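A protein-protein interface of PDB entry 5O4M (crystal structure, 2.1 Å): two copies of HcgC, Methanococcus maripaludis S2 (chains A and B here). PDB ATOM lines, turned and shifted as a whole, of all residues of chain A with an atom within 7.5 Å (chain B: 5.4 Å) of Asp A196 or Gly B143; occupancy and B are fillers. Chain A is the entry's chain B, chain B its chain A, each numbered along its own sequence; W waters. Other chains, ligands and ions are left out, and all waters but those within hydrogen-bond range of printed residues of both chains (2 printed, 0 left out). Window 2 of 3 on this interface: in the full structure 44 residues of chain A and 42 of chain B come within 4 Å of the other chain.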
ATOM      1  N   GLU A 191     -27.550 -36.349  -1.070  1.00  0.00           N
ATOM      2  CA  GLU A 191     -27.117 -36.912   0.200  1.00  0.00           C
ATOM      3  C   GLU A 191     -26.085 -36.041   0.893  1.00  0.00           C
ATOM      4  O   GLU A 191     -26.138 -35.895   2.106  1.00  0.00           O
ATOM      5  CB  GLU A 191     -26.576 -38.327  -0.020  1.00  0.00           C
ATOM      6  CG  GLU A 191     -26.244 -39.017   1.292  1.00  0.00           C
ATOM      7  CD  GLU A 191     -25.850 -40.472   1.165  1.00  0.00           C
ATOM      8  OE1 GLU A 191     -25.892 -41.022   0.037  1.00  0.00           O
ATOM      9  OE2 GLU A 191     -25.423 -41.037   2.197  1.00  0.00           O
ATOM     10  N   ILE A 192     -25.135 -35.469   0.141  1.00  0.00           N
ATOM     11  CA  ILE A 192     -24.108 -34.605   0.745  1.00  0.00           C
ATOM     12  C   ILE A 192     -24.749 -33.388   1.407  1.00  0.00           C
ATOM     13  O   ILE A 192     -24.299 -32.959   2.472  1.00  0.00           O
ATOM     14  CB  ILE A 192     -23.060 -34.183  -0.323  1.00  0.00           C
ATOM     15  CG1 ILE A 192     -22.147 -35.368  -0.677  1.00  0.00           C
ATOM     16  CG2 ILE A 192     -22.204 -32.966   0.140  1.00  0.00           C
ATOM     17  CD1 ILE A 192     -21.522 -35.269  -2.038  1.00  0.00           C
ATOM     18  N   ASN A 193     -25.800 -32.823   0.780  1.00  0.00           N
ATOM     19  CA  ASN A 193     -26.464 -31.652   1.335  1.00  0.00           C
ATOM     20  C   ASN A 193     -27.059 -31.896   2.718  1.00  0.00           C
ATOM     21  O   ASN A 193     -27.155 -30.969   3.520  1.00  0.00           O
ATOM     22  CB  ASN A 193     -27.497 -31.075   0.373  1.00  0.00           C
ATOM     23  CG  ASN A 193     -27.697 -29.605   0.582  1.00  0.00           C
ATOM     24  OD1 ASN A 193     -26.781 -28.835   0.374  1.00  0.00           O
ATOM     25  ND2 ASN A 193     -28.880 -29.168   0.998  1.00  0.00           N
ATOM     26  N   GLU A 194     -27.435 -33.140   2.996  1.00  0.00           N
ATOM     27  CA  GLU A 194     -28.004 -33.537   4.283  1.00  0.00           C
ATOM     28  C   GLU A 194     -26.950 -33.733   5.375  1.00  0.00           C
ATOM     29  O   GLU A 194     -27.325 -33.883   6.518  1.00  0.00           O
ATOM     30  CB  GLU A 194     -28.858 -34.785   4.126  1.00  0.00           C
ATOM     31  CG  GLU A 194     -30.064 -34.489   3.258  1.00  0.00           C
ATOM     32  CD  GLU A 194     -31.113 -35.582   3.255  1.00  0.00           C
ATOM     33  OE1 GLU A 194     -30.817 -36.693   3.756  1.00  0.00           O
ATOM     34  OE2 GLU A 194     -32.250 -35.302   2.807  1.00  0.00           O
ATOM     35  N   LEU A 195     -25.658 -33.723   5.054  1.00  0.00           N
ATOM     36  CA  LEU A 195     -24.633 -33.890   6.102  1.00  0.00           C
ATOM     37  C   LEU A 195     -24.739 -32.695   7.024  1.00  0.00           C
ATOM     38  O   LEU A 195     -25.083 -31.582   6.587  1.00  0.00           O
ATOM     39  CB  LEU A 195     -23.224 -33.963   5.505  1.00  0.00           C
ATOM     40  CG  LEU A 195     -22.920 -35.176   4.633  1.00  0.00           C
ATOM     41  CD1 LEU A 195     -21.635 -34.957   3.849  1.00  0.00           C
ATOM     42  CD2 LEU A 195     -22.824 -36.435   5.476  1.00  0.00           C
ATOM     43  N   ASP A 196     -24.461 -32.909   8.301  1.00  0.00           N
ATOM     44  CA  ASP A 196     -24.537 -31.834   9.279  1.00  0.00           C
ATOM     45  C   ASP A 196     -23.532 -30.727   8.934  1.00  0.00           C
ATOM     46  O   ASP A 196     -22.424 -31.013   8.498  1.00  0.00           O
ATOM     47  CB  ASP A 196     -24.318 -32.353  10.698  1.00  0.00           C
ATOM     48  CG  ASP A 196     -24.355 -31.246  11.745  1.00  0.00           C
ATOM     49  OD1 ASP A 196     -25.345 -30.461  11.750  1.00  0.00           O
ATOM     50  OD2 ASP A 196     -23.369 -31.131  12.525  1.00  0.00           O
ATOM     51  N   SER A 197     -23.947 -29.469   9.103  1.00  0.00           N
ATOM     52  CA  SER A 197     -23.149 -28.260   8.851  1.00  0.00           C
ATOM     53  C   SER A 197     -23.010 -27.828   7.370  1.00  0.00           C
ATOM     54  O   SER A 197     -22.455 -26.762   7.126  1.00  0.00           O
ATOM     55  CB  SER A 197     -21.770 -28.375   9.495  1.00  0.00           C
ATOM     56  OG  SER A 197     -20.774 -28.855   8.602  1.00  0.00           O
ATOM     57  N   VAL A 198     -23.513 -28.609   6.407  1.00  0.00           N
ATOM     58  CA  VAL A 198     -23.427 -28.238   5.003  1.00  0.00           C
ATOM     59  C   VAL A 198     -24.446 -27.106   4.719  1.00  0.00           C
ATOM     60  O   VAL A 198     -25.600 -27.213   5.130  1.00  0.00           O
ATOM     61  CB  VAL A 198     -23.632 -29.461   4.088  1.00  0.00           C
ATOM     62  CG1 VAL A 198     -23.772 -29.060   2.617  1.00  0.00           C
ATOM     63  CG2 VAL A 198     -22.489 -30.432   4.267  1.00  0.00           C
ATOM     64  N   LEU A 199     -24.002 -26.038   4.038  1.00  0.00           N
ATOM     65  CA  LEU A 199     -24.841 -24.899   3.678  1.00  0.00           C
ATOM     66  C   LEU A 199     -25.472 -25.226   2.345  1.00  0.00           C
ATOM     67  O   LEU A 199     -26.690 -25.199   2.228  1.00  0.00           O
ATOM     68  CB  LEU A 199     -24.049 -23.578   3.575  1.00  0.00           C
ATOM     69  CG  LEU A 199     -23.682 -22.908   4.902  1.00  0.00           C
ATOM     70  CD1 LEU A 199     -22.701 -23.696   5.672  1.00  0.00           C
ATOM     71  CD2 LEU A 199     -23.112 -21.558   4.660  1.00  0.00           C
ATOM     72  N   SER A 234     -19.535 -25.611   3.860  1.00  0.00           N
ATOM     73  CA  SER A 234     -19.944 -26.146   5.141  1.00  0.00           C
ATOM     74  C   SER A 234     -19.217 -25.499   6.307  1.00  0.00           C
ATOM     75  O   SER A 234     -18.166 -24.896   6.142  1.00  0.00           O
ATOM     76  CB  SER A 234     -19.689 -27.657   5.161  1.00  0.00           C
ATOM     77  OG  SER A 234     -18.303 -27.934   5.058  1.00  0.00           O
ATOM     78  N   ILE A 235     -19.772 -25.650   7.505  1.00  0.00           N
ATOM     79  CA  ILE A 235     -19.144 -25.102   8.703  1.00  0.00           C
ATOM     80  C   ILE A 235     -18.041 -26.082   9.155  1.00  0.00           C
ATOM     81  O   ILE A 235     -16.968 -25.648   9.542  1.00  0.00           O
ATOM     82  CB  ILE A 235     -20.159 -24.857   9.856  1.00  0.00           C
ATOM     83  CG1 ILE A 235     -21.381 -23.984   9.414  1.00  0.00           C
ATOM     84  CG2 ILE A 235     -19.477 -24.266  11.064  1.00  0.00           C
ATOM     85  CD1 ILE A 235     -21.033 -22.687   8.809  1.00  0.00           C
ATOM     86  N   ASP A 236     -18.331 -27.392   9.106  1.00  0.00           N
ATOM     87  CA  ASP A 236     -17.409 -28.449   9.537  1.00  0.00           C
ATOM     88  C   ASP A 236     -16.815 -29.231   8.389  1.00  0.00           C
ATOM     89  O   ASP A 236     -17.233 -29.106   7.234  1.00  0.00           O
ATOM     90  CB  ASP A 236     -18.148 -29.408  10.499  1.00  0.00           C
ATOM     91  CG  ASP A 236     -18.731 -28.724  11.735  1.00  0.00           C
ATOM     92  OD1 ASP A 236     -18.121 -27.738  12.215  1.00  0.00           O
ATOM     93  OD2 ASP A 236     -19.785 -29.188  12.230  1.00  0.00           O
ATOM     94  N   HIS A 237     -15.845 -30.065   8.711  1.00  0.00           N
ATOM     95  CA  HIS A 237     -15.183 -30.904   7.714  1.00  0.00           C
ATOM     96  C   HIS A 237     -16.150 -31.971   7.162  1.00  0.00           C
ATOM     97  O   HIS A 237     -16.796 -32.658   7.930  1.00  0.00           O
ATOM     98  CB  HIS A 237     -13.958 -31.619   8.333  1.00  0.00           C
ATOM     99  CG  HIS A 237     -12.811 -30.711   8.592  1.00  0.00           C
ATOM    100  ND1 HIS A 237     -11.797 -30.573   7.684  1.00  0.00           N
ATOM    101  CD2 HIS A 237     -12.543 -29.929   9.662  1.00  0.00           C
ATOM    102  CE1 HIS A 237     -10.955 -29.697   8.214  1.00  0.00           C
ATOM    103  NE2 HIS A 237     -11.363 -29.286   9.399  1.00  0.00           N
ATOM    104  N   VAL A 238     -16.255 -32.080   5.838  1.00  0.00           N
ATOM    105  CA  VAL A 238     -17.096 -33.060   5.150  1.00  0.00           C
ATOM    106  C   VAL A 238     -16.298 -33.785   4.104  1.00  0.00           C
ATOM    107  O   VAL A 238     -16.871 -34.568   3.354  1.00  0.00           O
ATOM    108  CB  VAL A 238     -18.343 -32.419   4.529  1.00  0.00           C
ATOM    109  CG1 VAL A 238     -19.246 -31.824   5.617  1.00  0.00           C
ATOM    110  CG2 VAL A 238     -17.989 -31.382   3.439  1.00  0.00           C
ATOM    111  N   GLU A 241     -16.648 -37.778   4.057  1.00  0.00           N
ATOM    112  CA  GLU A 241     -18.026 -38.178   3.727  1.00  0.00           C
ATOM    113  C   GLU A 241     -18.321 -37.875   2.282  1.00  0.00           C
ATOM    114  O   GLU A 241     -19.003 -38.644   1.616  1.00  0.00           O
ATOM    115  CB  GLU A 241     -19.060 -37.454   4.592  1.00  0.00           C
ATOM    116  CG  GLU A 241     -19.008 -37.813   6.063  1.00  0.00           C
ATOM    117  CD  GLU A 241     -18.093 -36.962   6.927  1.00  0.00           C
ATOM    118  OE1 GLU A 241     -17.118 -36.388   6.386  1.00  0.00           O
ATOM    119  OE2 GLU A 241     -18.328 -36.902   8.157  1.00  0.00           O
ATOM    120  N   ASP B 141     -30.540 -27.459  11.129  1.00  0.00           N
ATOM    121  CA  ASP B 141     -29.187 -28.002  11.001  1.00  0.00           C
ATOM    122  C   ASP B 141     -28.424 -27.563  12.249  1.00  0.00           C
ATOM    123  O   ASP B 141     -28.228 -26.369  12.447  1.00  0.00           O
ATOM    124  CB  ASP B 141     -28.490 -27.489   9.726  1.00  0.00           C
ATOM    125  CG  ASP B 141     -27.069 -28.039   9.586  1.00  0.00           C
ATOM    126  OD1 ASP B 141     -26.912 -29.128   9.002  1.00  0.00           O
ATOM    127  OD2 ASP B 141     -26.121 -27.371  10.058  1.00  0.00           O
ATOM    128  N   LYS B 142     -28.016 -28.503  13.081  1.00  0.00           N
ATOM    129  CA  LYS B 142     -27.286 -28.251  14.337  1.00  0.00           C
ATOM    130  C   LYS B 142     -25.991 -27.454  14.158  1.00  0.00           C
ATOM    131  O   LYS B 142     -25.717 -26.558  14.958  1.00  0.00           O
ATOM    132  CB  LYS B 142     -26.970 -29.559  15.073  1.00  0.00           C
ATOM    133  CG  LYS B 142     -28.200 -30.276  15.605  1.00  0.00           C
ATOM    134  CD  LYS B 142     -27.842 -31.601  16.239  1.00  0.00           C
ATOM    135  CE  LYS B 142     -28.995 -32.259  16.954  1.00  0.00           C
ATOM    136  NZ  LYS B 142     -28.613 -33.574  17.529  1.00  0.00           N
ATOM    137  N   GLY B 143     -25.220 -27.797  13.133  1.00  0.00           N
ATOM    138  CA  GLY B 143     -23.954 -27.146  12.814  1.00  0.00           C
ATOM    139  C   GLY B 143     -24.102 -25.669  12.524  1.00  0.00           C
ATOM    140  O   GLY B 143     -23.329 -24.841  13.027  1.00  0.00           O
ATOM    141  N   ILE B 144     -25.122 -25.332  11.723  1.00  0.00           N
ATOM    142  CA  ILE B 144     -25.405 -23.958  11.369  1.00  0.00           C
ATOM    143  C   ILE B 144     -26.002 -23.210  12.578  1.00  0.00           C
ATOM    144  O   ILE B 144     -25.669 -22.039  12.797  1.00  0.00           O
ATOM    145  CB  ILE B 144     -26.312 -23.880  10.108  1.00  0.00           C
ATOM    146  CG1 ILE B 144     -25.541 -24.351   8.867  1.00  0.00           C
ATOM    147  CG2 ILE B 144     -26.844 -22.449   9.908  1.00  0.00           C
ATOM    148  CD1 ILE B 144     -26.367 -24.871   7.752  1.00  0.00           C
ATOM    149  N   SER B 145     -26.888 -23.861  13.359  1.00  0.00           N
ATOM    150  CA  SER B 145     -27.488 -23.184  14.531  1.00  0.00           C
ATOM    151  C   SER B 145     -26.435 -22.803  15.551  1.00  0.00           C
ATOM    152  O   SER B 145     -26.513 -21.722  16.118  1.00  0.00           O
ATOM    153  CB  SER B 145     -28.567 -24.034  15.186  1.00  0.00           C
ATOM    154  OG  SER B 145     -29.746 -23.973  14.398  1.00  0.00           O
ATOM    155  N   LYS B 146     -25.452 -23.690  15.762  1.00  0.00           N
ATOM    156  CA  LYS B 146     -24.363 -23.479  16.699  1.00  0.00           C
ATOM    157  C   LYS B 146     -23.555 -22.213  16.362  1.00  0.00           C
ATOM    158  O   LYS B 146     -23.350 -21.372  17.242  1.00  0.00           O
ATOM    159  CB  LYS B 146     -23.442 -24.719  16.728  1.00  0.00           C
ATOM    160  CG  LYS B 146     -22.694 -24.915  18.025  1.00  0.00           C
ATOM    161  CD  LYS B 146     -21.817 -26.164  17.995  1.00  0.00           C
ATOM    162  CE  LYS B 146     -20.396 -25.908  17.574  1.00  0.00           C
ATOM    163  NZ  LYS B 146     -19.527 -25.503  18.702  1.00  0.00           N
ATOM    164  N   ILE B 147     -23.111 -22.080  15.103  1.00  0.00           N
ATOM    165  CA  ILE B 147     -22.320 -20.919  14.673  1.00  0.00           C
ATOM    166  C   ILE B 147     -23.158 -19.619  14.546  1.00  0.00           C
ATOM    167  O   ILE B 147     -22.585 -18.527  14.562  1.00  0.00           O
ATOM    168  CB  ILE B 147     -21.528 -21.242  13.373  1.00  0.00           C
ATOM    169  CG1 ILE B 147     -20.339 -20.250  13.183  1.00  0.00           C
ATOM    170  CG2 ILE B 147     -22.424 -21.282  12.109  1.00  0.00           C
ATOM    171  CD1 ILE B 147     -19.177 -20.833  12.514  1.00  0.00           C
ATOM    172  N   LYS B 173     -30.820 -25.315   3.733  1.00  0.00           N
ATOM    173  CA  LYS B 173     -29.955 -25.146   4.893  1.00  0.00           C
ATOM    174  C   LYS B 173     -29.776 -23.716   5.374  1.00  0.00           C
ATOM    175  O   LYS B 173     -29.581 -23.466   6.583  1.00  0.00           O
ATOM    176  CB  LYS B 173     -28.587 -25.757   4.612  1.00  0.00           C
ATOM    177  CG  LYS B 173     -28.611 -27.244   4.589  1.00  0.00           C
ATOM    178  CD  LYS B 173     -28.678 -27.820   6.011  1.00  0.00           C
ATOM    179  CE  LYS B 173     -28.353 -29.287   6.047  1.00  0.00           C
ATOM    180  NZ  LYS B 173     -26.915 -29.538   5.888  1.00  0.00           N
HETATM  181  O   HOH W   1     -29.419 -26.222   1.462  1.00  0.00           O
HETATM  182  O   HOH W   2     -23.018 -29.641  14.753  1.00  0.00           O
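No position is printed for both chains.
Of the 11 pairs that touch across the chains among the printed residues, none has its exchanged pair printed and touching as well.
The side-chain carboxylate (OD1) of Asp B141 lies within hydrogen-bond range of the backbone NH (N) of Ser A197.
The side-chain carboxylate (OD1) of Asp A196 sits at hydrogen-bond distance from the backbone NH (N) of Gly B143 (3.0 Å).
The backbone carbonyl oxygen (O) of Asn A193 sits at hydrogen-bond distance from the side-chain amino group (NZ) of Lys B173 (2.8 Å).
The side-chain amino group (NZ) of Lys B173 is in hydrogen-bond range of the backbone carbonyl oxygen (O) of Leu A195, at 2.8 Å.
NZ of Lys B173 is in hydrogen-bond range of O of Val A198.
The side-chain carboxylate (OD1) of Asp B141 sits close to the side-chain carboxylate (OD1) of Asp A196 (3.4 Å).
The side-chain carboxylate (OD2) of Asp B141 is in hydrogen-bond range of the backbone NH (N) of Gly B143, 3.2 Å away.
OD2 of Asp B141 lies within hydrogen-bond range of N of Ile B144, 2.8 Å away.
O of Asp B141 lies within hydrogen-bond range of OG of Ser B145, 3.4 Å away.
OD1 of Asp B141 lies within salt-bridge range of NZ of Lys B173 (3.1 Å).
The backbone NH (N) of Ile A235 is in hydrogen-bond range of the backbone carbonyl oxygen (O) of Ser A197, 2.9 Å away.
N of Asp A236 is in hydrogen-bond range of OG of Ser A197 (2.9 Å).
Among the printed residues, pairs that only touch across the chains: Leu A195 with Asp B141, Asp A196 with Lys B142, Val A198 with Ile B144, Leu A199 with Lys B173 and Ile A235 with Ile B147.
Of chain B, only Asp B141 (3.4 Å), Lys B142 (3.6 Å) and Gly B143 (3.0 Å) come within 4 Å of Asp A196.
Gly B143 touches one residue of chain A.
Of the printed residues of chain B, Leu A195 touches Asp B141 (3.9 Å) and Lys B173 (2.8 Å).
Of the printed residues of chain B, Asn A193 touches Lys B173.
Of the printed residues of chain A, Ile B144 touches Val A198 (3.6 Å).
Printed residues of chain B within 4 Å of Ile A235: Ile B147.
Of the printed residues of chain B, Val A198 touches Ile B144 and Lys B173.
Water W2 lies within hydrogen-bond range of OD2 of Asp A196 (2.7 Å) and N of Gly B143 (3.3 Å).
Water W1 lies within hydrogen-bond range of the backbone NH (N) of Lys B173 (2.8 Å), the backbone carbonyl oxygen (O) of Leu A199 (3.0 Å) and the side-chain amide nitrogen (ND2) of Asn A193 (3.0 Å).
Printed residues of chain A that touch a printed residue of chain B: Asn A193, Leu A195, Asp A196, Ser A197, Val A198, Leu A199 and Ile A235.
Along chain A the printed residues that touch a printed residue of chain B span positions 193 to 235.
Hydrophobic or aromatic side chains of chain B within 4 Å of the printed part of chain A: Ile B144 and Ile B147.
Among the printed residues, no Asp or Glu carboxylate lies within 4 Å of a Lys or Arg side-chain nitrogen of the other chain.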
